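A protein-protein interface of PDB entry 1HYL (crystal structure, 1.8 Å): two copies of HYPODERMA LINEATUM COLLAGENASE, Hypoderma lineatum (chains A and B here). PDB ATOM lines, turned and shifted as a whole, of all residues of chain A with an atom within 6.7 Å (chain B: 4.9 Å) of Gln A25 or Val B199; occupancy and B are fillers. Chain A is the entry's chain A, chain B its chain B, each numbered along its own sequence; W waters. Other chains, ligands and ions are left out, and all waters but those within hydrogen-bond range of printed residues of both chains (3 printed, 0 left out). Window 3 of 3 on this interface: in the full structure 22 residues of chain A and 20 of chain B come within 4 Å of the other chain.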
ATOM      1  N   THR A  21      -2.399 -16.395 -13.504  1.00  0.00           N
ATOM      2  CA  THR A  21      -2.046 -15.736 -14.750  1.00  0.00           C
ATOM      3  C   THR A  21      -1.458 -14.404 -14.289  1.00  0.00           C
ATOM      4  O   THR A  21      -2.033 -13.708 -13.433  1.00  0.00           O
ATOM      5  CB  THR A  21      -3.294 -15.505 -15.648  1.00  0.00           C
ATOM      6  OG1 THR A  21      -3.885 -16.769 -15.896  1.00  0.00           O
ATOM      7  CG2 THR A  21      -2.940 -14.933 -16.993  1.00  0.00           C
ATOM      8  N   LEU A  22      -0.286 -14.029 -14.791  1.00  0.00           N
ATOM      9  CA  LEU A  22       0.341 -12.829 -14.331  1.00  0.00           C
ATOM     10  C   LEU A  22       0.027 -11.682 -15.232  1.00  0.00           C
ATOM     11  O   LEU A  22      -0.518 -11.895 -16.320  1.00  0.00           O
ATOM     12  CB  LEU A  22       1.833 -12.984 -14.284  1.00  0.00           C
ATOM     13  CG  LEU A  22       2.452 -14.101 -13.473  1.00  0.00           C
ATOM     14  CD1 LEU A  22       3.926 -13.924 -13.590  1.00  0.00           C
ATOM     15  CD2 LEU A  22       2.011 -14.095 -12.022  1.00  0.00           C
ATOM     16  N   GLN A  23       0.411 -10.485 -14.793  1.00  0.00           N
ATOM     17  CA  GLN A  23       0.346  -9.272 -15.588  1.00  0.00           C
ATOM     18  C   GLN A  23       1.082  -9.418 -16.930  1.00  0.00           C
ATOM     19  O   GLN A  23       0.628  -8.880 -17.950  1.00  0.00           O
ATOM     20  CB  GLN A  23       0.963  -8.111 -14.820  1.00  0.00           C
ATOM     21  CG  GLN A  23      -0.101  -7.202 -14.252  1.00  0.00           C
ATOM     22  CD  GLN A  23       0.052  -6.895 -12.758  1.00  0.00           C
ATOM     23  OE1 GLN A  23      -0.871  -7.044 -11.942  1.00  0.00           O
ATOM     24  NE2 GLN A  23       1.247  -6.500 -12.334  1.00  0.00           N
ATOM     25  N   ASP A  24       2.169 -10.173 -17.023  1.00  0.00           N
ATOM     26  CA  ASP A  24       2.894 -10.342 -18.282  1.00  0.00           C
ATOM     27  C   ASP A  24       2.446 -11.515 -19.144  1.00  0.00           C
ATOM     28  O   ASP A  24       3.161 -11.969 -20.051  1.00  0.00           O
ATOM     29  CB  ASP A  24       4.387 -10.468 -17.944  1.00  0.00           C
ATOM     30  CG  ASP A  24       4.772 -11.623 -17.035  1.00  0.00           C
ATOM     31  OD1 ASP A  24       4.009 -12.550 -16.815  1.00  0.00           O
ATOM     32  OD2 ASP A  24       5.868 -11.596 -16.501  1.00  0.00           O
ATOM     33  N   GLN A  25       1.265 -12.035 -18.824  1.00  0.00           N
ATOM     34  CA  GLN A  25       0.594 -13.147 -19.479  1.00  0.00           C
ATOM     35  C   GLN A  25       1.155 -14.532 -19.194  1.00  0.00           C
ATOM     36  O   GLN A  25       0.656 -15.504 -19.753  1.00  0.00           O
ATOM     37  CB  GLN A  25       0.553 -12.932 -21.011  1.00  0.00           C
ATOM     38  CG  GLN A  25      -0.249 -11.642 -21.284  1.00  0.00           C
ATOM     39  CD  GLN A  25      -0.624 -11.291 -22.710  1.00  0.00           C
ATOM     40  OE1 GLN A  25      -0.280 -12.024 -23.621  1.00  0.00           O
ATOM     41  NE2 GLN A  25      -1.356 -10.226 -22.993  1.00  0.00           N
ATOM     42  N   ARG A  26       2.138 -14.767 -18.329  1.00  0.00           N
ATOM     43  CA  ARG A  26       2.585 -16.136 -18.028  1.00  0.00           C
ATOM     44  C   ARG A  26       1.701 -16.826 -17.009  1.00  0.00           C
ATOM     45  O   ARG A  26       0.997 -16.167 -16.232  1.00  0.00           O
ATOM     46  CB  ARG A  26       3.999 -16.165 -17.481  1.00  0.00           C
ATOM     47  CG  ARG A  26       5.019 -15.682 -18.468  1.00  0.00           C
ATOM     48  CD  ARG A  26       5.838 -14.781 -17.614  1.00  0.00           C
ATOM     49  NE  ARG A  26       7.149 -15.267 -17.466  1.00  0.00           N
ATOM     50  CZ  ARG A  26       8.082 -14.606 -16.789  1.00  0.00           C
ATOM     51  NH1 ARG A  26       7.925 -13.450 -16.154  1.00  0.00           N
ATOM     52  NH2 ARG A  26       9.256 -15.181 -16.805  1.00  0.00           N
ATOM     53  N   ARG A  27       1.752 -18.160 -17.065  1.00  0.00           N
ATOM     54  CA  ARG A  27       0.966 -19.076 -16.238  1.00  0.00           C
ATOM     55  C   ARG A  27       1.928 -19.668 -15.237  1.00  0.00           C
ATOM     56  O   ARG A  27       2.898 -20.327 -15.642  1.00  0.00           O
ATOM     57  CB  ARG A  27       0.363 -20.271 -17.011  1.00  0.00           C
ATOM     58  CG  ARG A  27      -1.085 -20.124 -17.340  1.00  0.00           C
ATOM     59  CD  ARG A  27      -1.852 -21.407 -17.019  1.00  0.00           C
ATOM     60  NE  ARG A  27      -1.756 -22.516 -17.949  1.00  0.00           N
ATOM     61  CZ  ARG A  27      -2.617 -23.553 -17.924  1.00  0.00           C
ATOM     62  NH1 ARG A  27      -3.511 -23.693 -16.945  1.00  0.00           N
ATOM     63  NH2 ARG A  27      -2.507 -24.513 -18.859  1.00  0.00           N
ATOM     64  N   TYR B  85       6.154  -5.587 -25.702  1.00  0.00           N
ATOM     65  CA  TYR B  85       6.523  -6.909 -26.217  1.00  0.00           C
ATOM     66  C   TYR B  85       7.368  -6.826 -27.482  1.00  0.00           C
ATOM     67  O   TYR B  85       7.388  -7.730 -28.317  1.00  0.00           O
ATOM     68  CB  TYR B  85       5.302  -7.760 -26.538  1.00  0.00           C
ATOM     69  CG  TYR B  85       4.606  -8.252 -25.290  1.00  0.00           C
ATOM     70  CD1 TYR B  85       5.070  -9.404 -24.649  1.00  0.00           C
ATOM     71  CD2 TYR B  85       3.515  -7.528 -24.802  1.00  0.00           C
ATOM     72  CE1 TYR B  85       4.423  -9.835 -23.492  1.00  0.00           C
ATOM     73  CE2 TYR B  85       2.868  -7.955 -23.651  1.00  0.00           C
ATOM     74  CZ  TYR B  85       3.330  -9.106 -23.006  1.00  0.00           C
ATOM     75  OH  TYR B  85       2.683  -9.522 -21.857  1.00  0.00           O
ATOM     76  N   TYR B 155      -5.538  -3.069 -31.648  1.00  0.00           N
ATOM     77  CA  TYR B 155      -4.680  -2.879 -30.459  1.00  0.00           C
ATOM     78  C   TYR B 155      -4.382  -1.435 -30.169  1.00  0.00           C
ATOM     79  O   TYR B 155      -4.725  -0.548 -30.960  1.00  0.00           O
ATOM     80  CB  TYR B 155      -3.320  -3.500 -30.693  1.00  0.00           C
ATOM     81  CG  TYR B 155      -3.342  -4.948 -30.336  1.00  0.00           C
ATOM     82  CD1 TYR B 155      -3.849  -5.853 -31.258  1.00  0.00           C
ATOM     83  CD2 TYR B 155      -2.873  -5.343 -29.091  1.00  0.00           C
ATOM     84  CE1 TYR B 155      -3.937  -7.193 -30.899  1.00  0.00           C
ATOM     85  CE2 TYR B 155      -2.946  -6.681 -28.737  1.00  0.00           C
ATOM     86  CZ  TYR B 155      -3.490  -7.606 -29.636  1.00  0.00           C
ATOM     87  OH  TYR B 155      -3.598  -8.908 -29.280  1.00  0.00           O
ATOM     88  N   PRO B 175      -4.834 -19.144 -29.428  1.00  0.00           N
ATOM     89  CA  PRO B 175      -3.798 -19.305 -28.393  1.00  0.00           C
ATOM     90  C   PRO B 175      -4.247 -18.669 -27.067  1.00  0.00           C
ATOM     91  O   PRO B 175      -5.018 -17.714 -27.073  1.00  0.00           O
ATOM     92  CB  PRO B 175      -2.591 -18.632 -28.995  1.00  0.00           C
ATOM     93  CG  PRO B 175      -2.850 -18.697 -30.490  1.00  0.00           C
ATOM     94  CD  PRO B 175      -4.330 -18.421 -30.579  1.00  0.00           C
ATOM     95  N   CYS B 176      -3.824 -19.126 -25.912  1.00  0.00           N
ATOM     96  CA  CYS B 176      -4.224 -18.491 -24.678  1.00  0.00           C
ATOM     97  C   CYS B 176      -3.062 -18.557 -23.738  1.00  0.00           C
ATOM     98  O   CYS B 176      -1.971 -18.889 -24.181  1.00  0.00           O
ATOM     99  CB  CYS B 176      -5.440 -19.207 -24.135  1.00  0.00           C
ATOM    100  SG  CYS B 176      -6.313 -18.203 -22.908  1.00  0.00           S
ATOM    101  N   PHE B 177      -3.176 -18.245 -22.457  1.00  0.00           N
ATOM    102  CA  PHE B 177      -2.049 -18.172 -21.532  1.00  0.00           C
ATOM    103  C   PHE B 177      -1.428 -19.537 -21.399  1.00  0.00           C
ATOM    104  O   PHE B 177      -2.143 -20.525 -21.234  1.00  0.00           O
ATOM    105  CB  PHE B 177      -2.546 -17.659 -20.166  1.00  0.00           C
ATOM    106  CG  PHE B 177      -3.295 -16.348 -20.381  1.00  0.00           C
ATOM    107  CD1 PHE B 177      -2.621 -15.236 -20.848  1.00  0.00           C
ATOM    108  CD2 PHE B 177      -4.669 -16.291 -20.190  1.00  0.00           C
ATOM    109  CE1 PHE B 177      -3.338 -14.086 -21.131  1.00  0.00           C
ATOM    110  CE2 PHE B 177      -5.371 -15.134 -20.478  1.00  0.00           C
ATOM    111  CZ  PHE B 177      -4.707 -14.025 -20.954  1.00  0.00           C
ATOM    112  N   GLY B 178      -0.102 -19.623 -21.515  1.00  0.00           N
ATOM    113  CA  GLY B 178       0.590 -20.895 -21.506  1.00  0.00           C
ATOM    114  C   GLY B 178       1.067 -21.268 -22.915  1.00  0.00           C
ATOM    115  O   GLY B 178       1.995 -22.078 -23.037  1.00  0.00           O
ATOM    116  N   SER B 180       2.392 -19.104 -25.000  1.00  0.00           N
ATOM    117  CA  SER B 180       3.602 -18.284 -25.148  1.00  0.00           C
ATOM    118  C   SER B 180       4.852 -18.981 -25.641  1.00  0.00           C
ATOM    119  O   SER B 180       5.164 -20.058 -25.140  1.00  0.00           O
ATOM    120  CB  SER B 180       3.942 -17.685 -23.825  1.00  0.00           C
ATOM    121  OG  SER B 180       3.025 -16.662 -23.498  1.00  0.00           O
ATOM    122  N   SER B 197       3.416 -14.480 -28.898  1.00  0.00           N
ATOM    123  CA  SER B 197       3.913 -13.402 -28.102  1.00  0.00           C
ATOM    124  C   SER B 197       2.855 -12.839 -27.202  1.00  0.00           C
ATOM    125  O   SER B 197       3.137 -12.759 -26.013  1.00  0.00           O
ATOM    126  CB  SER B 197       4.427 -12.352 -29.055  1.00  0.00           C
ATOM    127  OG  SER B 197       4.879 -11.157 -28.455  1.00  0.00           O
ATOM    128  N   PHE B 198       1.668 -12.420 -27.624  1.00  0.00           N
ATOM    129  CA  PHE B 198       0.769 -11.767 -26.692  1.00  0.00           C
ATOM    130  C   PHE B 198      -0.626 -11.918 -27.166  1.00  0.00           C
ATOM    131  O   PHE B 198      -0.895 -11.994 -28.353  1.00  0.00           O
ATOM    132  CB  PHE B 198       1.033 -10.248 -26.520  1.00  0.00           C
ATOM    133  CG  PHE B 198       1.194  -9.408 -27.786  1.00  0.00           C
ATOM    134  CD1 PHE B 198       0.100  -8.854 -28.434  1.00  0.00           C
ATOM    135  CD2 PHE B 198       2.463  -9.231 -28.326  1.00  0.00           C
ATOM    136  CE1 PHE B 198       0.301  -8.143 -29.613  1.00  0.00           C
ATOM    137  CE2 PHE B 198       2.647  -8.524 -29.495  1.00  0.00           C
ATOM    138  CZ  PHE B 198       1.568  -7.978 -30.145  1.00  0.00           C
ATOM    139  N   VAL B 199      -1.509 -12.020 -26.208  1.00  0.00           N
ATOM    140  CA  VAL B 199      -2.937 -12.124 -26.401  1.00  0.00           C
ATOM    141  C   VAL B 199      -3.450 -10.698 -26.132  1.00  0.00           C
ATOM    142  O   VAL B 199      -2.758  -9.818 -25.578  1.00  0.00           O
ATOM    143  CB  VAL B 199      -3.429 -13.195 -25.371  1.00  0.00           C
ATOM    144  CG1 VAL B 199      -4.923 -13.175 -25.240  1.00  0.00           C
ATOM    145  CG2 VAL B 199      -3.037 -14.604 -25.849  1.00  0.00           C
ATOM    146  N   SER B 200      -4.656 -10.450 -26.596  1.00  0.00           N
ATOM    147  CA  SER B 200      -5.343  -9.207 -26.400  1.00  0.00           C
ATOM    148  C   SER B 200      -5.572  -8.961 -24.935  1.00  0.00           C
ATOM    149  O   SER B 200      -5.793  -9.874 -24.141  1.00  0.00           O
ATOM    150  CB  SER B 200      -6.679  -9.257 -27.081  1.00  0.00           C
ATOM    151  OG  SER B 200      -7.290  -7.986 -26.914  1.00  0.00           O
ATOM    152  N   GLY B 201      -5.589  -7.687 -24.589  1.00  0.00           N
ATOM    153  CA  GLY B 201      -6.000  -7.274 -23.256  1.00  0.00           C
ATOM    154  C   GLY B 201      -7.427  -7.777 -22.977  1.00  0.00           C
ATOM    155  O   GLY B 201      -7.773  -8.111 -21.843  1.00  0.00           O
ATOM    156  N   GLY B 203      -8.462 -10.684 -23.465  1.00  0.00           N
ATOM    157  CA  GLY B 203      -8.485 -12.102 -23.209  1.00  0.00           C
ATOM    158  C   GLY B 203      -8.544 -12.862 -24.525  1.00  0.00           C
ATOM    159  O   GLY B 203      -8.536 -12.343 -25.652  1.00  0.00           O
ATOM    160  N   CYS B 204      -8.679 -14.149 -24.272  1.00  0.00           N
ATOM    161  CA  CYS B 204      -8.561 -15.195 -25.270  1.00  0.00           C
ATOM    162  C   CYS B 204      -9.821 -15.494 -26.037  1.00  0.00           C
ATOM    163  O   CYS B 204      -9.774 -15.924 -27.190  1.00  0.00           O
ATOM    164  CB  CYS B 204      -8.082 -16.506 -24.600  1.00  0.00           C
ATOM    165  SG  CYS B 204      -6.543 -16.361 -23.638  1.00  0.00           S
ATOM    166  N   VAL B 210      -4.031 -12.150 -32.273  1.00  0.00           N
ATOM    167  CA  VAL B 210      -2.963 -12.500 -31.343  1.00  0.00           C
ATOM    168  C   VAL B 210      -1.725 -12.009 -32.034  1.00  0.00           C
ATOM    169  O   VAL B 210      -1.649 -12.073 -33.258  1.00  0.00           O
ATOM    170  CB  VAL B 210      -2.912 -14.051 -31.102  1.00  0.00           C
ATOM    171  CG1 VAL B 210      -1.628 -14.598 -30.421  1.00  0.00           C
ATOM    172  CG2 VAL B 210      -4.083 -14.317 -30.169  1.00  0.00           C
HETATM  173  O   HOH W   1       0.916 -14.756 -24.118  1.00  0.00           O
HETATM  174  O   HOH W   2       1.869 -17.487 -21.274  1.00  0.00           O
HETATM  175  O   HOH W   3       0.637  -7.971 -20.544  1.00  0.00           O
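Water W2 lies within hydrogen-bond range of OG of Ser B180, O of Gln A25 and N of Gly B178.
Water W3 bridges the backbone carbonyl oxygen (O) of Gln A23 (2.7 Å) and the side-chain hydroxyl (OH) of Tyr B85 (2.9 Å).
Water W1 lies within hydrogen-bond range of the side-chain hydroxyl of Ser B180 (2.9 Å) and the side-chain amide oxygen of Gln A25 (3.0 Å).
The side-chain sulfur (SG) of Cys B204 is disulfide-bonded to the side-chain sulfur (SG) of Cys B176 (2.0 Å).
OD2 of Asp A24 is in salt-bridge range of NH1 of Arg A26.
No position is printed for both chains.
Of the 7 pairs that touch across the chains among the printed residues, none has its exchanged pair printed and touching as well.
Phe B177 touches Thr A21.
Gln A25 touches Tyr B85.
Phe B177 touches Gln A25.
OE1 of Gln A25 touches CA of Phe B198 (3.3 Å).
Phe B177 touches Arg A27 (O to NE, 3.9 Å).
Of the 15 printed residues of chain B, 4 touch a printed residue of chain A.
Printed residues of chain B that touch a printed residue of chain A: Tyr B85, Phe B177, Phe B198 and Val B199.
Hydrophobic or aromatic side chains of chain B that line the printed part of chain A: Tyr B85, Phe B177, Phe B198 and Val B199.
Leu A22 touches none of the printed residues of chain B.
Printed residues of chain B within 4 Å of Arg A27: Phe B177.
Printed residues of chain A within 4 Å of Phe B177: Thr A21, Gln A25 and Arg A27.
Printed residues of chain A within 4 Å of Phe B198: Gln A25 (3.3 Å).
Of chain A, only Gln A25 comes within 4 Å of Val B199.
Val B210 touches none of the printed residues of chain A.
The nearest printed residue of chain A that does not touch Tyr B85 is Gln A23 (4.5 Å).
OE1 of Gln A25 sits at hydrogen-bond distance from N of Val B199.
The side-chain hydroxyl (OH) of Tyr B85 lies within hydrogen-bond range of the backbone carbonyl oxygen (O) of Asp A24, at 3.1 Å.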
